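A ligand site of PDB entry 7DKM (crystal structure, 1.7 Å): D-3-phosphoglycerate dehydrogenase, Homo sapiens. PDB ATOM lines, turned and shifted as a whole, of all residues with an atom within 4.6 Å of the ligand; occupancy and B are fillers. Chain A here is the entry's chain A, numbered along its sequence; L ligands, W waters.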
ATOM      1  N   THR A  76     -18.542 -15.690 -18.561  1.00  0.00           N
ATOM      2  CA  THR A  76     -17.273 -15.594 -19.340  1.00  0.00           C
ATOM      3  C   THR A  76     -16.948 -16.930 -19.993  1.00  0.00           C
ATOM      4  O   THR A  76     -16.666 -16.934 -21.210  1.00  0.00           O
ATOM      5  CB  THR A  76     -16.096 -15.106 -18.477  1.00  0.00           C
ATOM      6  OG1 THR A  76     -16.426 -13.839 -17.900  1.00  0.00           O
ATOM      7  CG2 THR A  76     -14.816 -14.942 -19.270  1.00  0.00           C
ATOM      8  N   PRO A  97     -17.862 -11.138 -21.949  1.00  0.00           N
ATOM      9  CA  PRO A  97     -16.466 -10.986 -21.513  1.00  0.00           C
ATOM     10  C   PRO A  97     -16.198  -9.811 -20.562  1.00  0.00           C
ATOM     11  O   PRO A  97     -15.126  -9.830 -20.006  1.00  0.00           O
ATOM     12  CB  PRO A  97     -15.713 -10.805 -22.841  1.00  0.00           C
ATOM     13  CG  PRO A  97     -16.736 -10.241 -23.807  1.00  0.00           C
ATOM     14  CD  PRO A  97     -18.023 -10.900 -23.391  1.00  0.00           C
ATOM     15  N   ASN A 100     -18.162  -9.843 -15.873  1.00  0.00           N
ATOM     16  CA  ASN A 100     -17.571 -10.580 -14.716  1.00  0.00           C
ATOM     17  C   ASN A 100     -16.208 -10.024 -14.303  1.00  0.00           C
ATOM     18  O   ASN A 100     -15.676 -10.489 -13.276  1.00  0.00           O
ATOM     19  CB  ASN A 100     -17.381 -12.060 -15.032  1.00  0.00           C
ATOM     20  CG  ASN A 100     -18.685 -12.824 -15.000  1.00  0.00           C
ATOM     21  OD1 ASN A 100     -19.625 -12.427 -14.317  1.00  0.00           O
ATOM     22  ND2 ASN A 100     -18.737 -13.926 -15.730  1.00  0.00           N
ATOM     23  N   ALA A 104     -14.348 -10.859 -10.664  1.00  0.00           N
ATOM     24  CA  ALA A 104     -13.201 -11.800 -10.708  1.00  0.00           C
ATOM     25  C   ALA A 104     -11.938 -11.107 -10.171  1.00  0.00           C
ATOM     26  O   ALA A 104     -11.200 -11.724  -9.384  1.00  0.00           O
ATOM     27  CB  ALA A 104     -13.017 -12.344 -12.097  1.00  0.00           C
ATOM     28  N   LEU A 149       0.138 -12.803 -14.912  1.00  0.00           N
ATOM     29  CA  LEU A 149       0.223 -13.483 -16.232  1.00  0.00           C
ATOM     30  C   LEU A 149      -1.139 -13.348 -16.903  1.00  0.00           C
ATOM     31  O   LEU A 149      -2.114 -13.954 -16.416  1.00  0.00           O
ATOM     32  CB  LEU A 149       0.673 -14.927 -16.032  1.00  0.00           C
ATOM     33  CG  LEU A 149       1.884 -15.122 -15.119  1.00  0.00           C
ATOM     34  CD1 LEU A 149       2.327 -16.571 -15.111  1.00  0.00           C
ATOM     35  CD2 LEU A 149       3.041 -14.231 -15.545  1.00  0.00           C
ATOM     36  N   GLY A 150      -1.201 -12.535 -17.954  1.00  0.00           N
ATOM     37  CA  GLY A 150      -2.455 -12.144 -18.620  1.00  0.00           C
ATOM     38  C   GLY A 150      -2.843 -10.759 -18.172  1.00  0.00           C
ATOM     39  O   GLY A 150      -3.202 -10.586 -17.007  1.00  0.00           O
ATOM     40  N   LEU A 151      -2.707  -9.788 -19.068  1.00  0.00           N
ATOM     41  CA  LEU A 151      -2.904  -8.343 -18.785  1.00  0.00           C
ATOM     42  C   LEU A 151      -4.071  -7.841 -19.630  1.00  0.00           C
ATOM     43  O   LEU A 151      -3.979  -6.718 -20.154  1.00  0.00           O
ATOM     44  CB  LEU A 151      -1.594  -7.608 -19.070  1.00  0.00           C
ATOM     45  CG  LEU A 151      -0.371  -8.140 -18.314  1.00  0.00           C
ATOM     46  CD1 LEU A 151       0.895  -7.420 -18.760  1.00  0.00           C
ATOM     47  CD2 LEU A 151      -0.562  -7.996 -16.810  1.00  0.00           C
ATOM     48  N   GLY A 152      -5.130  -8.653 -19.710  1.00  0.00           N
ATOM     49  CA  GLY A 152      -6.391  -8.280 -20.362  1.00  0.00           C
ATOM     50  C   GLY A 152      -7.305  -7.585 -19.375  1.00  0.00           C
ATOM     51  O   GLY A 152      -6.807  -6.830 -18.501  1.00  0.00           O
ATOM     52  N   ARG A 153      -8.600  -7.858 -19.471  1.00  0.00           N
ATOM     53  CA  ARG A 153      -9.649  -7.177 -18.659  1.00  0.00           C
ATOM     54  C   ARG A 153      -9.351  -7.333 -17.172  1.00  0.00           C
ATOM     55  O   ARG A 153      -9.345  -6.324 -16.460  1.00  0.00           O
ATOM     56  CB  ARG A 153     -11.019  -7.746 -18.986  1.00  0.00           C
ATOM     57  CG  ARG A 153     -11.481  -7.447 -20.400  1.00  0.00           C
ATOM     58  CD  ARG A 153     -12.688  -8.274 -20.714  1.00  0.00           C
ATOM     59  NE  ARG A 153     -13.209  -7.983 -22.035  1.00  0.00           N
ATOM     60  CZ  ARG A 153     -12.750  -8.499 -23.161  1.00  0.00           C
ATOM     61  NH1 ARG A 153     -11.734  -9.348 -23.153  1.00  0.00           N
ATOM     62  NH2 ARG A 153     -13.311  -8.161 -24.319  1.00  0.00           N
ATOM     63  N   ILE A 154      -9.122  -8.562 -16.711  1.00  0.00           N
ATOM     64  CA  ILE A 154      -9.019  -8.835 -15.243  1.00  0.00           C
ATOM     65  C   ILE A 154      -7.605  -8.500 -14.759  1.00  0.00           C
ATOM     66  O   ILE A 154      -7.492  -7.850 -13.699  1.00  0.00           O
ATOM     67  CB  ILE A 154      -9.456 -10.266 -14.905  1.00  0.00           C
ATOM     68  CG1 ILE A 154     -10.931 -10.464 -15.285  1.00  0.00           C
ATOM     69  CG2 ILE A 154      -9.197 -10.559 -13.431  1.00  0.00           C
ATOM     70  CD1 ILE A 154     -11.408 -11.895 -15.261  1.00  0.00           C
ATOM     71  N   GLY A 155      -6.573  -8.903 -15.499  1.00  0.00           N
ATOM     72  CA  GLY A 155      -5.172  -8.658 -15.091  1.00  0.00           C
ATOM     73  C   GLY A 155      -4.922  -7.197 -14.747  1.00  0.00           C
ATOM     74  O   GLY A 155      -4.311  -6.926 -13.713  1.00  0.00           O
ATOM     75  N   TYR A 172       3.346 -10.494 -17.822  1.00  0.00           N
ATOM     76  CA  TYR A 172       3.597 -10.988 -19.183  1.00  0.00           C
ATOM     77  C   TYR A 172       2.254 -11.156 -19.882  1.00  0.00           C
ATOM     78  O   TYR A 172       1.305 -11.697 -19.284  1.00  0.00           O
ATOM     79  CB  TYR A 172       4.392 -12.294 -19.136  1.00  0.00           C
ATOM     80  CG  TYR A 172       4.553 -12.930 -20.494  1.00  0.00           C
ATOM     81  CD1 TYR A 172       5.515 -12.482 -21.387  1.00  0.00           C
ATOM     82  CD2 TYR A 172       3.708 -13.940 -20.907  1.00  0.00           C
ATOM     83  CE1 TYR A 172       5.631 -13.040 -22.650  1.00  0.00           C
ATOM     84  CE2 TYR A 172       3.807 -14.506 -22.157  1.00  0.00           C
ATOM     85  CZ  TYR A 172       4.771 -14.054 -23.037  1.00  0.00           C
ATOM     86  OH  TYR A 172       4.877 -14.632 -24.269  1.00  0.00           O
ATOM     87  N   ASP A 173       2.193 -10.686 -21.124  1.00  0.00           N
ATOM     88  CA  ASP A 173       1.063 -10.900 -22.058  1.00  0.00           C
ATOM     89  C   ASP A 173       1.633 -10.872 -23.469  1.00  0.00           C
ATOM     90  O   ASP A 173       2.301  -9.912 -23.833  1.00  0.00           O
ATOM     91  CB  ASP A 173      -0.003  -9.819 -21.843  1.00  0.00           C
ATOM     92  CG  ASP A 173      -1.318 -10.123 -22.544  1.00  0.00           C
ATOM     93  OD1 ASP A 173      -1.282 -10.406 -23.777  1.00  0.00           O
ATOM     94  OD2 ASP A 173      -2.352 -10.087 -21.862  1.00  0.00           O
ATOM     95  N   PRO A 174       1.416 -11.916 -24.295  1.00  0.00           N
ATOM     96  CA  PRO A 174       2.012 -11.961 -25.630  1.00  0.00           C
ATOM     97  C   PRO A 174       1.469 -10.900 -26.605  1.00  0.00           C
ATOM     98  O   PRO A 174       2.134 -10.669 -27.598  1.00  0.00           O
ATOM     99  CB  PRO A 174       1.701 -13.388 -26.116  1.00  0.00           C
ATOM    100  CG  PRO A 174       0.453 -13.774 -25.361  1.00  0.00           C
ATOM    101  CD  PRO A 174       0.588 -13.102 -24.006  1.00  0.00           C
ATOM    102  N   ILE A 175       0.306 -10.290 -26.328  1.00  0.00           N
ATOM    103  CA  ILE A 175      -0.336  -9.325 -27.275  1.00  0.00           C
ATOM    104  C   ILE A 175      -0.320  -7.883 -26.727  1.00  0.00           C
ATOM    105  O   ILE A 175      -0.447  -6.957 -27.540  1.00  0.00           O
ATOM    106  CB  ILE A 175      -1.762  -9.767 -27.674  1.00  0.00           C
ATOM    107  CG1 ILE A 175      -2.775  -9.614 -26.538  1.00  0.00           C
ATOM    108  CG2 ILE A 175      -1.723 -11.177 -28.233  1.00  0.00           C
ATOM    109  CD1 ILE A 175      -4.204  -9.709 -27.007  1.00  0.00           C
ATOM    110  N   ILE A 176      -0.174  -7.683 -25.423  1.00  0.00           N
ATOM    111  CA  ILE A 176      -0.170  -6.308 -24.831  1.00  0.00           C
ATOM    112  C   ILE A 176       1.262  -5.759 -24.888  1.00  0.00           C
ATOM    113  O   ILE A 176       2.157  -6.414 -24.367  1.00  0.00           O
ATOM    114  CB  ILE A 176      -0.766  -6.321 -23.405  1.00  0.00           C
ATOM    115  CG1 ILE A 176      -2.178  -6.911 -23.340  1.00  0.00           C
ATOM    116  CG2 ILE A 176      -0.714  -4.921 -22.820  1.00  0.00           C
ATOM    117  CD1 ILE A 176      -3.224  -6.120 -24.108  1.00  0.00           C
ATOM    118  N   HIS A 204      -4.382 -14.795 -15.234  1.00  0.00           N
ATOM    119  CA  HIS A 204      -5.589 -14.184 -15.836  1.00  0.00           C
ATOM    120  C   HIS A 204      -5.546 -14.377 -17.364  1.00  0.00           C
ATOM    121  O   HIS A 204      -5.775 -13.389 -18.105  1.00  0.00           O
ATOM    122  CB  HIS A 204      -5.712 -12.731 -15.381  1.00  0.00           C
ATOM    123  CG  HIS A 204      -5.757 -12.613 -13.906  1.00  0.00           C
ATOM    124  ND1 HIS A 204      -6.868 -13.013 -13.168  1.00  0.00           N
ATOM    125  CD2 HIS A 204      -4.819 -12.245 -12.994  1.00  0.00           C
ATOM    126  CE1 HIS A 204      -6.627 -12.834 -11.887  1.00  0.00           C
ATOM    127  NE2 HIS A 204      -5.367 -12.375 -11.750  1.00  0.00           N
ATOM    128  N   THR A 205      -5.281 -15.607 -17.786  1.00  0.00           N
ATOM    129  CA  THR A 205      -5.206 -16.009 -19.221  1.00  0.00           C
ATOM    130  C   THR A 205      -6.398 -16.888 -19.566  1.00  0.00           C
ATOM    131  O   THR A 205      -7.017 -17.465 -18.681  1.00  0.00           O
ATOM    132  CB  THR A 205      -3.894 -16.761 -19.501  1.00  0.00           C
ATOM    133  OG1 THR A 205      -3.971 -18.020 -18.843  1.00  0.00           O
ATOM    134  CG2 THR A 205      -2.667 -15.996 -19.031  1.00  0.00           C
ATOM    135  N   PRO A 206      -6.716 -17.052 -20.869  1.00  0.00           N
ATOM    136  CA  PRO A 206      -7.598 -18.129 -21.287  1.00  0.00           C
ATOM    137  C   PRO A 206      -6.880 -19.465 -21.040  1.00  0.00           C
ATOM    138  O   PRO A 206      -5.686 -19.451 -20.750  1.00  0.00           O
ATOM    139  CB  PRO A 206      -7.837 -17.891 -22.784  1.00  0.00           C
ATOM    140  CG  PRO A 206      -6.679 -17.024 -23.233  1.00  0.00           C
ATOM    141  CD  PRO A 206      -6.196 -16.262 -22.009  1.00  0.00           C
ATOM    142  N   LEU A 207      -7.627 -20.564 -21.101  1.00  0.00           N
ATOM    143  CA  LEU A 207      -7.062 -21.935 -21.118  1.00  0.00           C
ATOM    144  C   LEU A 207      -6.781 -22.290 -22.583  1.00  0.00           C
ATOM    145  O   LEU A 207      -7.739 -22.422 -23.366  1.00  0.00           O
ATOM    146  CB  LEU A 207      -8.012 -22.930 -20.456  1.00  0.00           C
ATOM    147  CG  LEU A 207      -7.473 -24.354 -20.358  1.00  0.00           C
ATOM    148  CD1 LEU A 207      -6.260 -24.411 -19.440  1.00  0.00           C
ATOM    149  CD2 LEU A 207      -8.564 -25.304 -19.873  1.00  0.00           C
ATOM    150  N   LEU A 208      -5.487 -22.365 -22.930  1.00  0.00           N
ATOM    151  CA  LEU A 208      -4.987 -22.719 -24.273  1.00  0.00           C
ATOM    152  C   LEU A 208      -3.883 -23.756 -24.075  1.00  0.00           C
ATOM    153  O   LEU A 208      -3.393 -23.904 -22.968  1.00  0.00           O
ATOM    154  CB  LEU A 208      -4.416 -21.461 -24.946  1.00  0.00           C
ATOM    155  CG  LEU A 208      -5.385 -20.289 -25.106  1.00  0.00           C
ATOM    156  CD1 LEU A 208      -4.635 -19.034 -25.523  1.00  0.00           C
ATOM    157  CD2 LEU A 208      -6.460 -20.623 -26.118  1.00  0.00           C
ATOM    158  N   SER A 210      -0.868 -23.274 -24.792  1.00  0.00           N
ATOM    159  CA  SER A 210       0.246 -22.410 -24.311  1.00  0.00           C
ATOM    160  C   SER A 210       0.095 -22.094 -22.809  1.00  0.00           C
ATOM    161  O   SER A 210       1.131 -21.804 -22.181  1.00  0.00           O
ATOM    162  CB  SER A 210       0.325 -21.155 -25.138  1.00  0.00           C
ATOM    163  OG  SER A 210      -0.925 -20.480 -25.150  1.00  0.00           O
ATOM    164  N   THR A 211      -1.115 -22.163 -22.241  1.00  0.00           N
ATOM    165  CA  THR A 211      -1.377 -21.800 -20.818  1.00  0.00           C
ATOM    166  C   THR A 211      -1.714 -23.033 -19.972  1.00  0.00           C
ATOM    167  O   THR A 211      -1.887 -22.874 -18.757  1.00  0.00           O
ATOM    168  CB  THR A 211      -2.455 -20.723 -20.704  1.00  0.00           C
ATOM    169  OG1 THR A 211      -3.692 -21.274 -21.145  1.00  0.00           O
ATOM    170  CG2 THR A 211      -2.111 -19.487 -21.500  1.00  0.00           C
ATOM    171  N   LEU A 214       0.919 -23.471 -17.435  1.00  0.00           N
ATOM    172  CA  LEU A 214       1.701 -22.208 -17.502  1.00  0.00           C
ATOM    173  C   LEU A 214       2.610 -22.133 -16.264  1.00  0.00           C
ATOM    174  O   LEU A 214       3.780 -21.690 -16.414  1.00  0.00           O
ATOM    175  CB  LEU A 214       0.734 -21.023 -17.563  1.00  0.00           C
ATOM    176  CG  LEU A 214       1.363 -19.643 -17.729  1.00  0.00           C
ATOM    177  CD1 LEU A 214       2.168 -19.563 -19.028  1.00  0.00           C
ATOM    178  CD2 LEU A 214       0.303 -18.563 -17.701  1.00  0.00           C
ATOM    179  N   CYS A 232      -7.616 -17.761 -10.122  1.00  0.00           N
ATOM    180  CA  CYS A 232      -9.048 -17.379 -10.282  1.00  0.00           C
ATOM    181  C   CYS A 232      -9.389 -17.255 -11.768  1.00  0.00           C
ATOM    182  O   CYS A 232     -10.296 -16.483 -12.098  1.00  0.00           O
ATOM    183  CB  CYS A 232      -9.362 -16.077  -9.554  1.00  0.00           C
ATOM    184  SG  CYS A 232      -9.304 -16.226  -7.749  1.00  0.00           S
ATOM    185  N   ALA A 233      -8.700 -18.000 -12.640  1.00  0.00           N
ATOM    186  CA  ALA A 233      -8.894 -17.941 -14.115  1.00  0.00           C
ATOM    187  C   ALA A 233      -9.608 -19.221 -14.574  1.00  0.00           C
ATOM    188  O   ALA A 233     -10.844 -19.202 -14.607  1.00  0.00           O
ATOM    189  CB  ALA A 233      -7.567 -17.710 -14.815  1.00  0.00           C
ATOM    190  N   ARG A 234      -8.868 -20.283 -14.879  1.00  0.00           N
ATOM    191  CA  ARG A 234      -9.432 -21.580 -15.341  1.00  0.00           C
ATOM    192  C   ARG A 234      -8.568 -22.716 -14.780  1.00  0.00           C
ATOM    193  O   ARG A 234      -7.335 -22.567 -14.714  1.00  0.00           O
ATOM    194  CB  ARG A 234      -9.508 -21.628 -16.863  1.00  0.00           C
ATOM    195  CG  ARG A 234     -10.361 -20.529 -17.489  1.00  0.00           C
ATOM    196  CD  ARG A 234     -10.841 -20.836 -18.904  1.00  0.00           C
ATOM    197  NE  ARG A 234     -11.245 -19.619 -19.587  1.00  0.00           N
ATOM    198  CZ  ARG A 234     -11.121 -19.386 -20.886  1.00  0.00           C
ATOM    199  NH1 ARG A 234     -10.602 -20.312 -21.680  1.00  0.00           N
ATOM    200  NH2 ARG A 234     -11.520 -18.236 -21.388  1.00  0.00           N
ATOM    201  N   ASP A 258      -9.805 -20.786  -7.146  1.00  0.00           N
ATOM    202  CA  ASP A 258     -11.256 -20.631  -7.423  1.00  0.00           C
ATOM    203  C   ASP A 258     -11.702 -21.725  -8.409  1.00  0.00           C
ATOM    204  O   ASP A 258     -12.919 -21.961  -8.519  1.00  0.00           O
ATOM    205  CB  ASP A 258     -11.556 -19.240  -7.972  1.00  0.00           C
ATOM    206  CG  ASP A 258     -13.037 -18.937  -7.990  1.00  0.00           C
ATOM    207  OD1 ASP A 258     -13.696 -19.166  -6.946  1.00  0.00           O
ATOM    208  OD2 ASP A 258     -13.549 -18.508  -9.063  1.00  0.00           O
ATOM    209  N   VAL A 259     -10.757 -22.363  -9.097  1.00  0.00           N
ATOM    210  CA  VAL A 259     -11.027 -23.176 -10.309  1.00  0.00           C
ATOM    211  C   VAL A 259     -10.138 -24.417 -10.310  1.00  0.00           C
ATOM    212  O   VAL A 259      -9.042 -24.350  -9.730  1.00  0.00           O
ATOM    213  CB  VAL A 259     -10.843 -22.354 -11.593  1.00  0.00           C
ATOM    214  CG1 VAL A 259     -11.908 -21.271 -11.699  1.00  0.00           C
ATOM    215  CG2 VAL A 259      -9.436 -21.772 -11.685  1.00  0.00           C
ATOM    216  N   HIS A 281     -15.594 -21.953  -7.423  1.00  0.00           N
ATOM    217  CA  HIS A 281     -15.711 -21.184  -8.690  1.00  0.00           C
ATOM    218  C   HIS A 281     -16.673 -20.009  -8.466  1.00  0.00           C
ATOM    219  O   HIS A 281     -17.717 -19.956  -9.148  1.00  0.00           O
ATOM    220  CB  HIS A 281     -16.164 -22.111  -9.819  1.00  0.00           C
ATOM    221  CG  HIS A 281     -15.875 -21.595 -11.194  1.00  0.00           C
ATOM    222  ND1 HIS A 281     -15.590 -22.430 -12.247  1.00  0.00           N
ATOM    223  CD2 HIS A 281     -15.823 -20.338 -11.677  1.00  0.00           C
ATOM    224  CE1 HIS A 281     -15.392 -21.715 -13.331  1.00  0.00           C
ATOM    225  NE2 HIS A 281     -15.518 -20.427 -13.014  1.00  0.00           N
ATOM    226  N   LEU A 282     -16.330 -19.115  -7.542  1.00  0.00           N
ATOM    227  CA  LEU A 282     -17.155 -17.955  -7.141  1.00  0.00           C
ATOM    228  C   LEU A 282     -16.712 -16.667  -7.840  1.00  0.00           C
ATOM    229  O   LEU A 282     -17.276 -15.610  -7.516  1.00  0.00           O
ATOM    230  CB  LEU A 282     -17.056 -17.801  -5.616  1.00  0.00           C
ATOM    231  CG  LEU A 282     -17.654 -18.931  -4.790  1.00  0.00           C
ATOM    232  CD1 LEU A 282     -17.543 -18.610  -3.300  1.00  0.00           C
ATOM    233  CD2 LEU A 282     -19.100 -19.184  -5.174  1.00  0.00           C
ATOM    234  N   GLY A 283     -15.757 -16.714  -8.775  1.00  0.00           N
ATOM    235  CA  GLY A 283     -15.197 -15.499  -9.412  1.00  0.00           C
ATOM    236  C   GLY A 283     -16.264 -14.568  -9.986  1.00  0.00           C
ATOM    237  O   GLY A 283     -16.083 -13.332  -9.924  1.00  0.00           O
ATOM    238  N   ALA A 284     -17.352 -15.127 -10.537  1.00  0.00           N
ATOM    239  CA  ALA A 284     -18.450 -14.375 -11.175  1.00  0.00           C
ATOM    240  C   ALA A 284     -19.692 -14.358 -10.269  1.00  0.00           C
ATOM    241  O   ALA A 284     -20.761 -13.863 -10.703  1.00  0.00           O
ATOM    242  CB  ALA A 284     -18.753 -14.984 -12.522  1.00  0.00           C
HETATM  243  P1  LIG L   1      -9.029 -11.353 -21.580  1.00  0.00           P
HETATM  244  O1  LIG L   1      -9.262 -12.061 -22.858  1.00  0.00           O
HETATM  245  O2  LIG L   1      -9.560  -9.963 -21.447  1.00  0.00           O
HETATM  246  O3  LIG L   1      -7.486 -11.353 -21.206  1.00  0.00           O
HETATM  247  C1  LIG L   1      -6.717 -12.571 -21.299  1.00  0.00           C
HETATM  248  C2  LIG L   1      -5.314 -12.190 -21.652  1.00  0.00           C
HETATM  249  O4  LIG L   1      -4.461 -13.361 -21.526  1.00  0.00           O
HETATM  250  C3  LIG L   1      -5.120 -11.662 -23.091  1.00  0.00           C
HETATM  251  O5  LIG L   1      -4.654 -10.318 -23.081  1.00  0.00           O
HETATM  252  C4  LIG L   1      -4.150 -12.678 -23.711  1.00  0.00           C
HETATM  253  O6  LIG L   1      -3.239 -12.106 -24.640  1.00  0.00           O
HETATM  254  C5  LIG L   1      -3.446 -13.201 -22.470  1.00  0.00           C
HETATM  255  N1  LIG L   1      -2.691 -14.436 -22.668  1.00  0.00           N
HETATM  256  C6  LIG L   1      -2.882 -15.417 -23.620  1.00  0.00           C
HETATM  257  N2  LIG L   1      -1.965 -16.352 -23.594  1.00  0.00           N
HETATM  258  C7  LIG L   1      -1.098 -15.949 -22.578  1.00  0.00           C
HETATM  259  C8  LIG L   1       0.091 -16.514 -22.068  1.00  0.00           C
HETATM  260  N3  LIG L   1       0.660 -17.614 -22.551  1.00  0.00           N
HETATM  261  N4  LIG L   1       0.719 -15.834 -21.073  1.00  0.00           N
HETATM  262  C9  LIG L   1       0.162 -14.709 -20.606  1.00  0.00           C
HETATM  263  N5  LIG L   1      -0.944 -14.090 -21.018  1.00  0.00           N
HETATM  264  C10 LIG L   1      -1.539 -14.774 -22.017  1.00  0.00           C
HETATM  265  O7  LIG L   1      -9.629 -12.271 -20.414  1.00  0.00           O
HETATM  266  P2  LIG L   1     -10.213 -11.867 -18.991  1.00  0.00           P
HETATM  267  O8  LIG L   1     -11.592 -11.334 -19.173  1.00  0.00           O
HETATM  268  O9  LIG L   1      -9.207 -11.011 -18.290  1.00  0.00           O
HETATM  269  O10 LIG L   1     -10.289 -13.299 -18.284  1.00  0.00           O
HETATM  270  C11 LIG L   1      -9.074 -13.964 -17.860  1.00  0.00           C
HETATM  271  C12 LIG L   1      -9.397 -15.367 -17.421  1.00  0.00           C
HETATM  272  O11 LIG L   1     -10.272 -15.323 -16.267  1.00  0.00           O
HETATM  273  C13 LIG L   1     -10.130 -16.246 -18.447  1.00  0.00           C
HETATM  274  O12 LIG L   1      -9.635 -17.582 -18.390  1.00  0.00           O
HETATM  275  C14 LIG L   1     -11.580 -16.180 -17.978  1.00  0.00           C
HETATM  276  O13 LIG L   1     -12.362 -17.261 -18.432  1.00  0.00           O
HETATM  277  C15 LIG L   1     -11.345 -16.231 -16.467  1.00  0.00           C
HETATM  278  N6  LIG L   1     -12.499 -15.811 -15.638  1.00  0.00           N
HETATM  279  C16 LIG L   1     -12.813 -16.554 -14.528  1.00  0.00           C
HETATM  280  C17 LIG L   1     -13.895 -16.195 -13.731  1.00  0.00           C
HETATM  281  C18 LIG L   1     -14.168 -16.983 -12.480  1.00  0.00           C
HETATM  282  O14 LIG L   1     -15.330 -17.116 -12.131  1.00  0.00           O
HETATM  283  N7  LIG L   1     -13.124 -17.486 -11.817  1.00  0.00           N
HETATM  284  C19 LIG L   1     -14.712 -15.141 -14.126  1.00  0.00           C
HETATM  285  C20 LIG L   1     -14.303 -14.320 -15.154  1.00  0.00           C
HETATM  286  C21 LIG L   1     -13.219 -14.694 -15.918  1.00  0.00           C
HETATM  287  O   HOH W   1      -9.245 -14.340 -13.799  1.00  0.00           O
HETATM  288  O   HOH W   2     -13.369 -11.686 -20.965  1.00  0.00           O
HETATM  289  O   HOH W   3      -0.717 -18.013 -25.321  1.00  0.00           O
HETATM  290  O   HOH W   4      -8.688  -7.966 -23.204  1.00  0.00           O
HETATM  291  O   HOH W   5     -13.943 -11.075 -17.640  1.00  0.00           O
HETATM  292  O   HOH W   6     -12.385 -12.547 -23.425  1.00  0.00           O
HETATM  293  O   HOH W   7     -17.217 -17.870 -14.118  1.00  0.00           O
HETATM  294  O   HOH W   8      -6.510 -10.653 -18.038  1.00  0.00           O
HETATM  295  O   HOH W   9      -5.249 -15.382 -26.052  1.00  0.00           O
HETATM  296  O   HOH W  10     -15.243 -18.530 -15.730  1.00  0.00           O
HETATM  297  O   HOH W  11      -6.321  -8.626 -24.475  1.00  0.00           O
HETATM  298  O   HOH W  12      -4.106 -13.342 -27.022  1.00  0.00           O
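The side-chain carboxylate (OD2) of Asp 173 is in hydrogen-bond range of an oxygen (O5) of the ligand. O of Thr 205 sits at hydrogen-bond distance from O12 of the ligand. The backbone NH (N) of Arg 153 lies within hydrogen-bond range of an oxygen (O2) of the ligand. The guanidinium group (NH1) of Arg 153 lies within salt-bridge range of an oxygen (O2) of the ligand, 2.8 Å away. O13 of the ligand lies within hydrogen-bond range of NE of Arg 234 (2.9 Å). N of Ile 154 lies within hydrogen-bond range of O9 of the ligand. A nitrogen (N7) of the ligand is in hydrogen-bond range of the side-chain carboxylate of Asp 258. A nitrogen (N7) of the ligand sits at hydrogen-bond distance from the backbone carbonyl oxygen (O) of Cys 232, 3.0 Å away. The backbone NH (N) of Gly 283 lies close to an oxygen (O14) of the ligand (3.4 Å). O14 of the ligand sits at hydrogen-bond distance from N of Ala 284, at 3.3 Å. A ring nitrogen (NE2) of His 281 lies close to an oxygen (O14) of the ligand (3.4 Å). The backbone NH (N) of Gly 150 sits close to a nitrogen (N5) of the ligand (3.4 Å).
OD2 of Asp 173 sits at hydrogen-bond distance from N of Leu 151 (2.8 Å). The side-chain carboxylate of Asp 258 is in hydrogen-bond range of the backbone NH of Gly 283, 2.9 Å away. N of His 281 is in hydrogen-bond range of O of Asp 258 (2.9 Å). The side-chain carboxylate (OD1) of Asp 258 sits at hydrogen-bond distance from the backbone NH (N) of Leu 282, at 2.7 Å. O of Leu 149 is in hydrogen-bond range of N of His 204. The backbone NH of Gly 150 sits at hydrogen-bond distance from the backbone carbonyl oxygen of Tyr 172 (3.0 Å). The side-chain amide nitrogen of Asn 100 lies within hydrogen-bond range of the side-chain hydroxyl of Thr 76, at 3.2 Å. OG1 of Thr 211 sits at hydrogen-bond distance from N of Leu 208 (2.8 Å).
Merely in contact with the ligand: Thr 76 (3.5 Å), Pro 97 (3.9 Å), Asn 100 (3.8 Å), Ala 104 (3.8 Å), Gly 152 (3.4 Å), Tyr 172 (3.5 Å), Pro 174 (3.4 Å), Ile 175 (3.2 Å), His 204 (3.4 Å), Pro 206 (3.4 Å), Thr 211 (3.5 Å), Ala 233 (3.3 Å) and Val 259 (3.98 Å). Hydrophobic or aromatic side chains that line the ligand: Ala 104, Ile 154, Tyr 172, Pro 174, Ile 175, Pro 206, Ala 233, Val 259 and His 281. Of the 33 residues printed, 24 come within 4 Å of the ligand.
Water W2 lies within hydrogen-bond range of O8 of the ligand and O of Pro 97. Water W3 bridges OG of Ser 210 (2.5 Å) and N2 of the ligand (2.7 Å). Water W4 lies within hydrogen-bond range of O2 of the ligand and NH1 of Arg 153. Water W5 bridges an oxygen (O8) of the ligand (2.8 Å) and the backbone carbonyl oxygen of Pro 97 (2.9 Å). Water W7 bridges an oxygen (O14) of the ligand (2.8 Å) and a ring nitrogen (NE2) of His 281 (3.3 Å). Water W1 lies within hydrogen-bond range of ND1 of His 204 (2.8 Å), O11 of the ligand (2.8 Å) and O of Cys 232 (2.9 Å).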
